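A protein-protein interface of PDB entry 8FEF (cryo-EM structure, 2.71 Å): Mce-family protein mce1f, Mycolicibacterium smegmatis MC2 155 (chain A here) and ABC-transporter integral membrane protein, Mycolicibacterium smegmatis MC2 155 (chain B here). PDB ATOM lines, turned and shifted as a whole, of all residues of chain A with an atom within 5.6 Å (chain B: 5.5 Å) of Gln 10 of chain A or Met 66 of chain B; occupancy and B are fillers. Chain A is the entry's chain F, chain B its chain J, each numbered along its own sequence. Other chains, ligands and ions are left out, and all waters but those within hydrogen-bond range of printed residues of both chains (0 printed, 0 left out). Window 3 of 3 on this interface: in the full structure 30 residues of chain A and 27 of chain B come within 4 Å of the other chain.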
ATOM      1  N   PHE A   6     -12.238  16.048 -13.219  1.00  0.00           N
ATOM      2  CA  PHE A   6     -10.893  15.904 -13.760  1.00  0.00           C
ATOM      3  C   PHE A   6      -9.897  15.555 -12.661  1.00  0.00           C
ATOM      4  O   PHE A   6      -9.034  14.690 -12.853  1.00  0.00           O
ATOM      5  CB  PHE A   6     -10.472  17.190 -14.475  1.00  0.00           C
ATOM      6  CG  PHE A   6      -9.019  17.231 -14.848  1.00  0.00           C
ATOM      7  CD1 PHE A   6      -8.539  16.466 -15.897  1.00  0.00           C
ATOM      8  CD2 PHE A   6      -8.136  18.050 -14.161  1.00  0.00           C
ATOM      9  CE1 PHE A   6      -7.202  16.506 -16.248  1.00  0.00           C
ATOM     10  CE2 PHE A   6      -6.799  18.096 -14.508  1.00  0.00           C
ATOM     11  CZ  PHE A   6      -6.333  17.323 -15.553  1.00  0.00           C
ATOM     12  N   ILE A   7     -10.014  16.219 -11.509  1.00  0.00           N
ATOM     13  CA  ILE A   7      -9.300  15.780 -10.315  1.00  0.00           C
ATOM     14  C   ILE A   7      -9.717  14.361  -9.950  1.00  0.00           C
ATOM     15  O   ILE A   7      -8.892  13.542  -9.532  1.00  0.00           O
ATOM     16  CB  ILE A   7      -9.544  16.770  -9.160  1.00  0.00           C
ATOM     17  CG1 ILE A   7      -8.805  18.085  -9.420  1.00  0.00           C
ATOM     18  CG2 ILE A   7      -9.131  16.179  -7.822  1.00  0.00           C
ATOM     19  CD1 ILE A   7      -7.309  17.927  -9.559  1.00  0.00           C
ATOM     20  N   LYS A   8     -11.003  14.040 -10.129  1.00  0.00           N
ATOM     21  CA  LYS A   8     -11.474  12.679  -9.895  1.00  0.00           C
ATOM     22  C   LYS A   8     -10.820  11.694 -10.858  1.00  0.00           C
ATOM     23  O   LYS A   8     -10.453  10.579 -10.466  1.00  0.00           O
ATOM     24  CB  LYS A   8     -12.996  12.626 -10.021  1.00  0.00           C
ATOM     25  CG  LYS A   8     -13.620  11.320  -9.565  1.00  0.00           C
ATOM     26  CD  LYS A   8     -13.400  11.094  -8.081  1.00  0.00           C
ATOM     27  CE  LYS A   8     -14.245   9.941  -7.572  1.00  0.00           C
ATOM     28  NZ  LYS A   8     -14.012   8.696  -8.350  1.00  0.00           N
ATOM     29  N   MET A   9     -10.680  12.084 -12.129  1.00  0.00           N
ATOM     30  CA  MET A   9     -10.019  11.226 -13.108  1.00  0.00           C
ATOM     31  C   MET A   9      -8.559  10.994 -12.740  1.00  0.00           C
ATOM     32  O   MET A   9      -8.059   9.862 -12.819  1.00  0.00           O
ATOM     33  CB  MET A   9     -10.129  11.843 -14.502  1.00  0.00           C
ATOM     34  CG  MET A   9      -9.321  11.124 -15.569  1.00  0.00           C
ATOM     35  SD  MET A   9      -9.313  12.004 -17.142  1.00  0.00           S
ATOM     36  CE  MET A   9      -8.233  10.954 -18.111  1.00  0.00           C
ATOM     37  N   GLN A  10      -7.857  12.057 -12.339  1.00  0.00           N
ATOM     38  CA  GLN A  10      -6.479  11.899 -11.889  1.00  0.00           C
ATOM     39  C   GLN A  10      -6.404  10.986 -10.674  1.00  0.00           C
ATOM     40  O   GLN A  10      -5.507  10.141 -10.576  1.00  0.00           O
ATOM     41  CB  GLN A  10      -5.866  13.263 -11.572  1.00  0.00           C
ATOM     42  CG  GLN A  10      -5.569  14.116 -12.791  1.00  0.00           C
ATOM     43  CD  GLN A  10      -4.730  15.332 -12.453  1.00  0.00           C
ATOM     44  OE1 GLN A  10      -4.527  15.653 -11.283  1.00  0.00           O
ATOM     45  NE2 GLN A  10      -4.227  16.008 -13.478  1.00  0.00           N
ATOM     46  N   LEU A  11      -7.352  11.131  -9.746  1.00  0.00           N
ATOM     47  CA  LEU A  11      -7.356  10.306  -8.544  1.00  0.00           C
ATOM     48  C   LEU A  11      -7.554   8.834  -8.883  1.00  0.00           C
ATOM     49  O   LEU A  11      -6.854   7.968  -8.346  1.00  0.00           O
ATOM     50  CB  LEU A  11      -8.447  10.789  -7.591  1.00  0.00           C
ATOM     51  CG  LEU A  11      -8.164  10.674  -6.095  1.00  0.00           C
ATOM     52  CD1 LEU A  11      -6.968  11.530  -5.721  1.00  0.00           C
ATOM     53  CD2 LEU A  11      -9.386  11.079  -5.291  1.00  0.00           C
ATOM     54  N   VAL A  12      -8.498   8.528  -9.777  1.00  0.00           N
ATOM     55  CA  VAL A  12      -8.776   7.127 -10.087  1.00  0.00           C
ATOM     56  C   VAL A  12      -7.631   6.505 -10.885  1.00  0.00           C
ATOM     57  O   VAL A  12      -7.275   5.340 -10.661  1.00  0.00           O
ATOM     58  CB  VAL A  12     -10.140   6.962 -10.789  1.00  0.00           C
ATOM     59  CG1 VAL A  12     -11.261   7.444  -9.881  1.00  0.00           C
ATOM     60  CG2 VAL A  12     -10.190   7.677 -12.124  1.00  0.00           C
ATOM     61  N   ILE A  13      -7.028   7.253 -11.818  1.00  0.00           N
ATOM     62  CA  ILE A  13      -5.902   6.683 -12.555  1.00  0.00           C
ATOM     63  C   ILE A  13      -4.702   6.488 -11.629  1.00  0.00           C
ATOM     64  O   ILE A  13      -3.974   5.491 -11.738  1.00  0.00           O
ATOM     65  CB  ILE A  13      -5.553   7.527 -13.800  1.00  0.00           C
ATOM     66  CG1 ILE A  13      -4.519   6.796 -14.662  1.00  0.00           C
ATOM     67  CG2 ILE A  13      -5.022   8.899 -13.439  1.00  0.00           C
ATOM     68  CD1 ILE A  13      -4.103   7.559 -15.901  1.00  0.00           C
ATOM     69  N   PHE A  14      -4.493   7.413 -10.684  1.00  0.00           N
ATOM     70  CA  PHE A  14      -3.423   7.239  -9.711  1.00  0.00           C
ATOM     71  C   PHE A  14      -3.675   6.030  -8.820  1.00  0.00           C
ATOM     72  O   PHE A  14      -2.741   5.300  -8.480  1.00  0.00           O
ATOM     73  CB  PHE A  14      -3.262   8.505  -8.869  1.00  0.00           C
ATOM     74  CG  PHE A  14      -2.349   8.330  -7.693  1.00  0.00           C
ATOM     75  CD1 PHE A  14      -0.976   8.361  -7.858  1.00  0.00           C
ATOM     76  CD2 PHE A  14      -2.863   8.135  -6.422  1.00  0.00           C
ATOM     77  CE1 PHE A  14      -0.134   8.196  -6.780  1.00  0.00           C
ATOM     78  CE2 PHE A  14      -2.026   7.969  -5.340  1.00  0.00           C
ATOM     79  CZ  PHE A  14      -0.661   7.997  -5.520  1.00  0.00           C
ATOM     80  N   LEU A  15      -4.930   5.807  -8.422  1.00  0.00           N
ATOM     81  CA  LEU A  15      -5.244   4.647  -7.592  1.00  0.00           C
ATOM     82  C   LEU A  15      -5.044   3.343  -8.358  1.00  0.00           C
ATOM     83  O   LEU A  15      -4.571   2.350  -7.792  1.00  0.00           O
ATOM     84  CB  LEU A  15      -6.675   4.748  -7.066  1.00  0.00           C
ATOM     85  CG  LEU A  15      -7.062   3.732  -5.989  1.00  0.00           C
ATOM     86  CD1 LEU A  15      -6.207   3.923  -4.748  1.00  0.00           C
ATOM     87  CD2 LEU A  15      -8.538   3.845  -5.648  1.00  0.00           C
ATOM     88  N   VAL B  61      -3.866  15.503  -3.288  1.00  0.00           N
ATOM     89  CA  VAL B  61      -3.344  14.179  -3.620  1.00  0.00           C
ATOM     90  C   VAL B  61      -3.309  13.996  -5.131  1.00  0.00           C
ATOM     91  O   VAL B  61      -2.305  13.546  -5.696  1.00  0.00           O
ATOM     92  CB  VAL B  61      -4.179  13.079  -2.939  1.00  0.00           C
ATOM     93  CG1 VAL B  61      -3.922  11.733  -3.591  1.00  0.00           C
ATOM     94  CG2 VAL B  61      -3.854  13.005  -1.463  1.00  0.00           C
ATOM     95  N   ALA B  62      -4.402  14.357  -5.805  1.00  0.00           N
ATOM     96  CA  ALA B  62      -4.438  14.248  -7.262  1.00  0.00           C
ATOM     97  C   ALA B  62      -3.400  15.157  -7.911  1.00  0.00           C
ATOM     98  O   ALA B  62      -2.715  14.753  -8.858  1.00  0.00           O
ATOM     99  CB  ALA B  62      -5.837  14.574  -7.779  1.00  0.00           C
ATOM    100  N   GLU B  63      -3.269  16.388  -7.408  1.00  0.00           N
ATOM    101  CA  GLU B  63      -2.335  17.347  -7.990  1.00  0.00           C
ATOM    102  C   GLU B  63      -0.889  16.896  -7.819  1.00  0.00           C
ATOM    103  O   GLU B  63      -0.074  17.051  -8.734  1.00  0.00           O
ATOM    104  CB  GLU B  63      -2.548  18.722  -7.359  1.00  0.00           C
ATOM    105  CG  GLU B  63      -1.788  19.850  -8.029  1.00  0.00           C
ATOM    106  CD  GLU B  63      -2.122  21.202  -7.432  1.00  0.00           C
ATOM    107  OE1 GLU B  63      -2.792  21.237  -6.380  1.00  0.00           O
ATOM    108  OE2 GLU B  63      -1.715  22.229  -8.015  1.00  0.00           O
ATOM    109  N   ILE B  64      -0.549  16.350  -6.651  1.00  0.00           N
ATOM    110  CA  ILE B  64       0.810  15.872  -6.419  1.00  0.00           C
ATOM    111  C   ILE B  64       1.084  14.617  -7.237  1.00  0.00           C
ATOM    112  O   ILE B  64       2.154  14.476  -7.841  1.00  0.00           O
ATOM    113  CB  ILE B  64       1.039  15.639  -4.915  1.00  0.00           C
ATOM    114  CG1 ILE B  64       1.042  16.971  -4.164  1.00  0.00           C
ATOM    115  CG2 ILE B  64       2.339  14.902  -4.675  1.00  0.00           C
ATOM    116  CD1 ILE B  64       1.299  16.836  -2.684  1.00  0.00           C
ATOM    117  N   GLY B  65       0.126  13.687  -7.278  1.00  0.00           N
ATOM    118  CA  GLY B  65       0.346  12.445  -7.998  1.00  0.00           C
ATOM    119  C   GLY B  65       0.458  12.631  -9.499  1.00  0.00           C
ATOM    120  O   GLY B  65       1.292  11.996 -10.149  1.00  0.00           O
ATOM    121  N   MET B  66      -0.372  13.500 -10.075  1.00  0.00           N
ATOM    122  CA  MET B  66      -0.421  13.657 -11.523  1.00  0.00           C
ATOM    123  C   MET B  66       0.102  15.011 -11.993  1.00  0.00           C
ATOM    124  O   MET B  66      -0.138  15.397 -13.142  1.00  0.00           O
ATOM    125  CB  MET B  66      -1.845  13.426 -12.025  1.00  0.00           C
ATOM    126  CG  MET B  66      -2.431  12.092 -11.591  1.00  0.00           C
ATOM    127  SD  MET B  66      -1.353  10.694 -11.965  1.00  0.00           S
ATOM    128  CE  MET B  66      -1.258  10.799 -13.750  1.00  0.00           C
ATOM    129  N   GLY B  67       0.807  15.739 -11.135  1.00  0.00           N
ATOM    130  CA  GLY B  67       1.459  16.969 -11.545  1.00  0.00           C
ATOM    131  C   GLY B  67       0.483  18.113 -11.755  1.00  0.00           C
ATOM    132  O   GLY B  67      -0.735  17.980 -11.640  1.00  0.00           O
ATOM    133  N   THR B  68       1.054  19.271 -12.081  1.00  0.00           N
ATOM    134  CA  THR B  68       0.274  20.471 -12.337  1.00  0.00           C
ATOM    135  C   THR B  68       0.996  21.319 -13.374  1.00  0.00           C
ATOM    136  O   THR B  68       2.203  21.180 -13.586  1.00  0.00           O
ATOM    137  CB  THR B  68       0.038  21.281 -11.055  1.00  0.00           C
ATOM    138  OG1 THR B  68      -0.673  22.485 -11.370  1.00  0.00           O
ATOM    139  CG2 THR B  68       1.362  21.638 -10.399  1.00  0.00           C
ATOM    140  N   MET B  71       3.861  20.549 -16.705  1.00  0.00           N
ATOM    141  CA  MET B  71       4.455  19.252 -16.410  1.00  0.00           C
ATOM    142  C   MET B  71       3.419  18.156 -16.203  1.00  0.00           C
ATOM    143  O   MET B  71       3.788  16.978 -16.171  1.00  0.00           O
ATOM    144  CB  MET B  71       5.350  19.355 -15.172  1.00  0.00           C
ATOM    145  CG  MET B  71       6.680  20.045 -15.433  1.00  0.00           C
ATOM    146  SD  MET B  71       7.531  20.525 -13.920  1.00  0.00           S
ATOM    147  CE  MET B  71       6.475  21.854 -13.357  1.00  0.00           C
ATOM    148  N   ALA B  72       2.141  18.509 -16.060  1.00  0.00           N
ATOM    149  CA  ALA B  72       1.109  17.505 -15.831  1.00  0.00           C
ATOM    150  C   ALA B  72       0.759  16.733 -17.096  1.00  0.00           C
ATOM    151  O   ALA B  72       0.313  15.583 -17.008  1.00  0.00           O
ATOM    152  CB  ALA B  72      -0.148  18.163 -15.261  1.00  0.00           C
ATOM    153  N   GLY B  75       2.650  13.412 -17.548  1.00  0.00           N
ATOM    154  CA  GLY B  75       2.503  12.403 -16.520  1.00  0.00           C
ATOM    155  C   GLY B  75       2.666  12.971 -15.127  1.00  0.00           C
ATOM    156  O   GLY B  75       2.181  12.392 -14.151  1.00  0.00           O
ATOM    157  N   GLY B  76       3.346  14.109 -15.023  1.00  0.00           N
ATOM    158  CA  GLY B  76       3.549  14.753 -13.743  1.00  0.00           C
ATOM    159  C   GLY B  76       4.688  14.156 -12.945  1.00  0.00           C
ATOM    160  O   GLY B  76       5.732  13.816 -13.505  1.00  0.00           O
ATOM    161  N   THR B  77       4.496  14.036 -11.630  1.00  0.00           N
ATOM    162  CA  THR B  77       5.531  13.471 -10.770  1.00  0.00           C
ATOM    163  C   THR B  77       5.823  12.016 -11.118  1.00  0.00           C
ATOM    164  O   THR B  77       6.971  11.570 -11.005  1.00  0.00           O
ATOM    165  CB  THR B  77       5.112  13.594  -9.304  1.00  0.00           C
ATOM    166  OG1 THR B  77       4.756  14.952  -9.021  1.00  0.00           O
ATOM    167  CG2 THR B  77       6.245  13.179  -8.379  1.00  0.00           C
ATOM    168  N   VAL B  78       4.805  11.272 -11.556  1.00  0.00           N
ATOM    169  CA  VAL B  78       4.980   9.850 -11.848  1.00  0.00           C
ATOM    170  C   VAL B  78       5.981   9.654 -12.979  1.00  0.00           C
ATOM    171  O   VAL B  78       6.891   8.822 -12.887  1.00  0.00           O
ATOM    172  CB  VAL B  78       3.623   9.199 -12.174  1.00  0.00           C
ATOM    173  CG1 VAL B  78       3.819   7.777 -12.668  1.00  0.00           C
ATOM    174  CG2 VAL B  78       2.730   9.210 -10.950  1.00  0.00           C
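O of Ala 62 of chain B lies close to OE1 of Gln 10 of chain A (3.2 Å).
CG2 of Ile 7 of chain A touches CB of Ala 62 of chain B, 3.7 Å away.
Gln 10 of chain A touches Met 66 of chain B (CD to CB, 3.5 Å).
Val 61 of chain B touches Leu 11 of chain A.
CD1 of Leu 11 of chain A touches N of Ala 62 of chain B, at 3.8 Å.
Printed residues of chain B within 4 Å of Ile 7 of chain A: Ala 62.
Of the printed residues of chain B, Gln 10 of chain A touches Ala 62 and Met 66.
Printed residues of chain B within 4 Å of Leu 11 of chain A: Val 61 (3.7 Å) and Ala 62 (3.8 Å).
Leu 15 of chain A touches none of the printed residues of chain B.
Printed residues of chain A within 4 Å of Val 61 of chain B: Leu 11 (3.7 Å).
Of the printed residues of chain A, Ala 62 of chain B touches Ile 7 (3.7 Å), Gln 10 (3.2 Å) and Leu 11 (3.8 Å).
The nearest residue of chain B that does not touch Gln 10 of chain A is Glu 63 of chain B (4.1 Å).
Hydrophobic or aromatic side chains of chain A within 4 Å of the printed part of chain B: Ile 7 and Leu 11.
Printed residues of chain B that touch a printed residue of chain A: Val 61, Ala 62 and Met 66.
Hydrophobic or aromatic side chains of chain B that line the printed part of chain A: Val 61, Ala 62 and Met 66.
Among the printed residues, 5 pairs touch across the chains.
Among the printed residues, no Asp or Glu carboxylate lies within 4 Å of a Lys or Arg side-chain nitrogen of the other chain.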
